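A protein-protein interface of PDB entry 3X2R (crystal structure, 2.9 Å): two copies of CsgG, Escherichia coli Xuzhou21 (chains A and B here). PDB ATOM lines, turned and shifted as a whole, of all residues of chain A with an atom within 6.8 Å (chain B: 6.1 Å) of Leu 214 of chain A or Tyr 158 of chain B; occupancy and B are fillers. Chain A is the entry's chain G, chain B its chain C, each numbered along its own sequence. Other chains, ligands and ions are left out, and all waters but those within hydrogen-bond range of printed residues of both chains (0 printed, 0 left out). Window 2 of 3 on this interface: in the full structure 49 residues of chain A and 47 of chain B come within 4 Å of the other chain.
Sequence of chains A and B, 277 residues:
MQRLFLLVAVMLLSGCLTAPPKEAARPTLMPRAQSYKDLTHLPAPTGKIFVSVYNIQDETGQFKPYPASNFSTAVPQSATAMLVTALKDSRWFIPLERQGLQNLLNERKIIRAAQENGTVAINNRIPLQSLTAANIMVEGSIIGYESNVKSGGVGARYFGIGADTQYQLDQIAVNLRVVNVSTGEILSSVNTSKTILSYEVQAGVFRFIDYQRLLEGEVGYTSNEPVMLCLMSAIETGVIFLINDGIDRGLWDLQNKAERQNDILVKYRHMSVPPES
N of Arg 157 of chain B lies within hydrogen-bond range of O of Glu 216 of chain A, 2.6 Å away. The backbone carbonyl oxygen (O) of Leu 214 of chain A is in hydrogen-bond range of the backbone NH (N) of Phe 159 of chain B, at 3.3 Å.
The backbone carbonyl oxygen of Leu 215 of chain A sits at hydrogen-bond distance from the backbone NH of Arg 207 of chain A, at 2.9 Å. The backbone NH (N) of Arg 213 of chain A sits at hydrogen-bond distance from the side-chain carboxylate (OD1) of Asp 210 of chain A (3.3 Å).
Among the printed residues, merely in contact across the chains: Arg 213 of chain A with Phe 159 of chain B (3.9 Å), Leu 214 of chain A with Tyr 158 of chain B (3.9 Å), Leu 215 of chain A with Arg 157 of chain B (3.5 Å), Leu 215 of chain A with Tyr 158 of chain B (3.7 Å) and Glu 216 of chain A with Ala 156 of chain B (3.6 Å).
Printed residues of chain B within 4 Å of Arg 213 of chain A: Phe 159. Leu 214 of chain A touches just these residues of chain B: Tyr 158 (3.9 Å) and Phe 159 (3.3 Å). Printed residues of chain B within 4 Å of Glu 216 of chain A: Ala 156 (3.6 Å) and Arg 157 (2.6 Å). Tyr 158 of chain B touches just these residues of chain A: Leu 214 and Leu 215. Gly 160 of chain B touches none of the printed residues of chain A. The nearest residue of chain B that does not touch Leu 214 of chain A is Arg 157 of chain B (4.3 Å).
Hydrophobic or aromatic side chains of chain A that line the printed part of chain B: Leu 214 and Leu 215. Among the printed residues, no Asp or Glu carboxylate lies within 4 Å of a Lys or Arg side-chain nitrogen of the other chain.
No position is printed for both chains.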
ATOM      1  N   ARG A 207      17.177 -14.506 -19.878  1.00  0.00           N
ATOM      2  CA  ARG A 207      15.825 -13.955 -19.878  1.00  0.00           C
ATOM      3  C   ARG A 207      15.768 -12.516 -20.393  1.00  0.00           C
ATOM      4  O   ARG A 207      16.690 -11.728 -20.174  1.00  0.00           O
ATOM      5  CB  ARG A 207      15.216 -14.036 -18.476  1.00  0.00           C
ATOM      6  N   PHE A 208      14.676 -12.182 -21.074  1.00  0.00           N
ATOM      7  CA  PHE A 208      14.467 -10.838 -21.605  1.00  0.00           C
ATOM      8  C   PHE A 208      13.348 -10.125 -20.852  1.00  0.00           C
ATOM      9  O   PHE A 208      12.380 -10.753 -20.424  1.00  0.00           O
ATOM     10  CB  PHE A 208      14.136 -10.894 -23.099  1.00  0.00           C
ATOM     11  CG  PHE A 208      15.241 -10.393 -23.987  1.00  0.00           C
ATOM     12  CD1 PHE A 208      16.366  -9.792 -23.448  1.00  0.00           C
ATOM     13  CD2 PHE A 208      15.149 -10.517 -25.364  1.00  0.00           C
ATOM     14  CE1 PHE A 208      17.383  -9.330 -24.265  1.00  0.00           C
ATOM     15  CE2 PHE A 208      16.161 -10.056 -26.186  1.00  0.00           C
ATOM     16  CZ  PHE A 208      17.279  -9.463 -25.636  1.00  0.00           C
ATOM     17  N   ILE A 209      13.485  -8.812 -20.688  1.00  0.00           N
ATOM     18  CA  ILE A 209      12.470  -8.020 -19.997  1.00  0.00           C
ATOM     19  C   ILE A 209      12.013  -6.813 -20.818  1.00  0.00           C
ATOM     20  O   ILE A 209      10.842  -6.720 -21.192  1.00  0.00           O
ATOM     21  CB  ILE A 209      12.964  -7.531 -18.619  1.00  0.00           C
ATOM     22  CG1 ILE A 209      13.334  -8.718 -17.726  1.00  0.00           C
ATOM     23  CG2 ILE A 209      11.904  -6.668 -17.948  1.00  0.00           C
ATOM     24  CD1 ILE A 209      13.841  -8.317 -16.359  1.00  0.00           C
ATOM     25  N   ASP A 210      12.943  -5.894 -21.076  1.00  0.00           N
ATOM     26  CA  ASP A 210      12.669  -4.663 -21.823  1.00  0.00           C
ATOM     27  C   ASP A 210      11.615  -3.797 -21.134  1.00  0.00           C
ATOM     28  O   ASP A 210      11.933  -3.002 -20.250  1.00  0.00           O
ATOM     29  CB  ASP A 210      12.259  -4.963 -23.271  1.00  0.00           C
ATOM     30  CG  ASP A 210      13.361  -5.638 -24.062  1.00  0.00           C
ATOM     31  OD1 ASP A 210      14.547  -5.348 -23.796  1.00  0.00           O
ATOM     32  OD2 ASP A 210      13.044  -6.456 -24.951  1.00  0.00           O
ATOM     33  N   ARG A 213      16.660  -3.799 -21.860  1.00  0.00           N
ATOM     34  CA  ARG A 213      16.937  -4.494 -20.608  1.00  0.00           C
ATOM     35  C   ARG A 213      17.017  -6.002 -20.825  1.00  0.00           C
ATOM     36  O   ARG A 213      16.577  -6.508 -21.859  1.00  0.00           O
ATOM     37  CB  ARG A 213      15.868  -4.168 -19.564  1.00  0.00           C
ATOM     38  N   LEU A 214      17.561  -6.709 -19.836  1.00  0.00           N
ATOM     39  CA  LEU A 214      17.755  -8.158 -19.912  1.00  0.00           C
ATOM     40  C   LEU A 214      18.321  -8.694 -18.601  1.00  0.00           C
ATOM     41  O   LEU A 214      18.777  -7.931 -17.750  1.00  0.00           O
ATOM     42  CB  LEU A 214      18.689  -8.534 -21.077  1.00  0.00           C
ATOM     43  CG  LEU A 214      20.220  -8.369 -21.065  1.00  0.00           C
ATOM     44  CD1 LEU A 214      20.692  -7.079 -20.387  1.00  0.00           C
ATOM     45  CD2 LEU A 214      20.930  -9.594 -20.483  1.00  0.00           C
ATOM     46  N   LEU A 215      18.279 -10.013 -18.444  1.00  0.00           N
ATOM     47  CA  LEU A 215      18.801 -10.661 -17.248  1.00  0.00           C
ATOM     48  C   LEU A 215      19.467 -11.969 -17.647  1.00  0.00           C
ATOM     49  O   LEU A 215      18.938 -12.716 -18.466  1.00  0.00           O
ATOM     50  CB  LEU A 215      17.677 -10.919 -16.237  1.00  0.00           C
ATOM     51  CG  LEU A 215      18.045 -11.209 -14.777  1.00  0.00           C
ATOM     52  CD1 LEU A 215      16.882 -10.850 -13.865  1.00  0.00           C
ATOM     53  CD2 LEU A 215      18.445 -12.665 -14.567  1.00  0.00           C
ATOM     54  N   GLU A 216      20.630 -12.246 -17.069  1.00  0.00           N
ATOM     55  CA  GLU A 216      21.306 -13.514 -17.313  1.00  0.00           C
ATOM     56  C   GLU A 216      22.188 -13.925 -16.141  1.00  0.00           C
ATOM     57  O   GLU A 216      22.656 -13.079 -15.380  1.00  0.00           O
ATOM     58  CB  GLU A 216      22.116 -13.464 -18.613  1.00  0.00           C
ATOM     59  CG  GLU A 216      23.288 -12.501 -18.595  1.00  0.00           C
ATOM     60  CD  GLU A 216      24.336 -12.835 -19.642  1.00  0.00           C
ATOM     61  OE1 GLU A 216      25.368 -12.135 -19.702  1.00  0.00           O
ATOM     62  OE2 GLU A 216      24.128 -13.801 -20.406  1.00  0.00           O
ATOM     63  N   ALA B 156      26.732 -13.383 -12.703  1.00  0.00           N
ATOM     64  CA  ALA B 156      25.382 -12.939 -13.014  1.00  0.00           C
ATOM     65  C   ALA B 156      25.417 -11.587 -13.710  1.00  0.00           C
ATOM     66  O   ALA B 156      26.312 -10.782 -13.469  1.00  0.00           O
ATOM     67  CB  ALA B 156      24.550 -12.861 -11.748  1.00  0.00           C
ATOM     68  N   ARG B 157      24.449 -11.345 -14.585  1.00  0.00           N
ATOM     69  CA  ARG B 157      24.351 -10.053 -15.246  1.00  0.00           C
ATOM     70  C   ARG B 157      22.911  -9.563 -15.335  1.00  0.00           C
ATOM     71  O   ARG B 157      22.039 -10.242 -15.876  1.00  0.00           O
ATOM     72  CB  ARG B 157      24.979 -10.117 -16.641  1.00  0.00           C
ATOM     73  CG  ARG B 157      24.733  -8.891 -17.509  1.00  0.00           C
ATOM     74  CD  ARG B 157      25.308  -9.094 -18.903  1.00  0.00           C
ATOM     75  NE  ARG B 157      24.902  -8.048 -19.837  1.00  0.00           N
ATOM     76  CZ  ARG B 157      25.606  -6.948 -20.080  1.00  0.00           C
ATOM     77  NH1 ARG B 157      26.760  -6.747 -19.460  1.00  0.00           N
ATOM     78  NH2 ARG B 157      25.159  -6.051 -20.949  1.00  0.00           N
ATOM     79  N   TYR B 158      22.674  -8.378 -14.786  1.00  0.00           N
ATOM     80  CA  TYR B 158      21.394  -7.701 -14.918  1.00  0.00           C
ATOM     81  C   TYR B 158      21.684  -6.366 -15.583  1.00  0.00           C
ATOM     82  O   TYR B 158      22.808  -5.875 -15.506  1.00  0.00           O
ATOM     83  CB  TYR B 158      20.760  -7.489 -13.545  1.00  0.00           C
ATOM     84  CG  TYR B 158      19.440  -6.752 -13.575  1.00  0.00           C
ATOM     85  CD1 TYR B 158      18.271  -7.390 -13.968  1.00  0.00           C
ATOM     86  CD2 TYR B 158      19.361  -5.417 -13.195  1.00  0.00           C
ATOM     87  CE1 TYR B 158      17.062  -6.717 -13.995  1.00  0.00           C
ATOM     88  CE2 TYR B 158      18.158  -4.737 -13.216  1.00  0.00           C
ATOM     89  CZ  TYR B 158      17.012  -5.392 -13.615  1.00  0.00           C
ATOM     90  OH  TYR B 158      15.813  -4.717 -13.637  1.00  0.00           O
ATOM     91  N   PHE B 159      20.687  -5.779 -16.235  1.00  0.00           N
ATOM     92  CA  PHE B 159      20.908  -4.529 -16.955  1.00  0.00           C
ATOM     93  C   PHE B 159      21.124  -3.363 -15.995  1.00  0.00           C
ATOM     94  O   PHE B 159      20.276  -3.082 -15.149  1.00  0.00           O
ATOM     95  CB  PHE B 159      19.742  -4.230 -17.902  1.00  0.00           C
ATOM     96  CG  PHE B 159      19.890  -2.937 -18.657  1.00  0.00           C
ATOM     97  CD1 PHE B 159      20.679  -2.870 -19.796  1.00  0.00           C
ATOM     98  CD2 PHE B 159      19.232  -1.791 -18.234  1.00  0.00           C
ATOM     99  CE1 PHE B 159      20.817  -1.683 -20.494  1.00  0.00           C
ATOM    100  CE2 PHE B 159      19.367  -0.602 -18.929  1.00  0.00           C
ATOM    101  CZ  PHE B 159      20.160  -0.548 -20.061  1.00  0.00           C
ATOM    102  N   GLY B 160      22.260  -2.685 -16.130  1.00  0.00           N
ATOM    103  CA  GLY B 160      23.297  -3.086 -17.066  1.00  0.00           C
ATOM    104  C   GLY B 160      24.519  -3.639 -16.357  1.00  0.00           C
ATOM    105  O   GLY B 160      25.575  -3.821 -16.965  1.00  0.00           O
ATOM    106  N   ILE B 161      24.368  -3.913 -15.064  1.00  0.00           N
ATOM    107  CA  ILE B 161      25.496  -4.289 -14.216  1.00  0.00           C
ATOM    108  C   ILE B 161      25.700  -5.798 -14.094  1.00  0.00           C
ATOM    109  O   ILE B 161      24.890  -6.501 -13.493  1.00  0.00           O
ATOM    110  CB  ILE B 161      25.338  -3.712 -12.789  1.00  0.00           C
ATOM    111  CG1 ILE B 161      25.165  -2.189 -12.830  1.00  0.00           C
ATOM    112  CG2 ILE B 161      26.529  -4.094 -11.925  1.00  0.00           C
ATOM    113  CD1 ILE B 161      23.721  -1.720 -12.792  1.00  0.00           C
ATOM    114  N   GLY B 162      26.789  -6.288 -14.677  1.00  0.00           N
ATOM    115  CA  GLY B 162      27.217  -7.662 -14.493  1.00  0.00           C
ATOM    116  C   GLY B 162      28.349  -7.796 -13.486  1.00  0.00           C
ATOM    117  O   GLY B 162      29.049  -6.827 -13.190  1.00  0.00           O
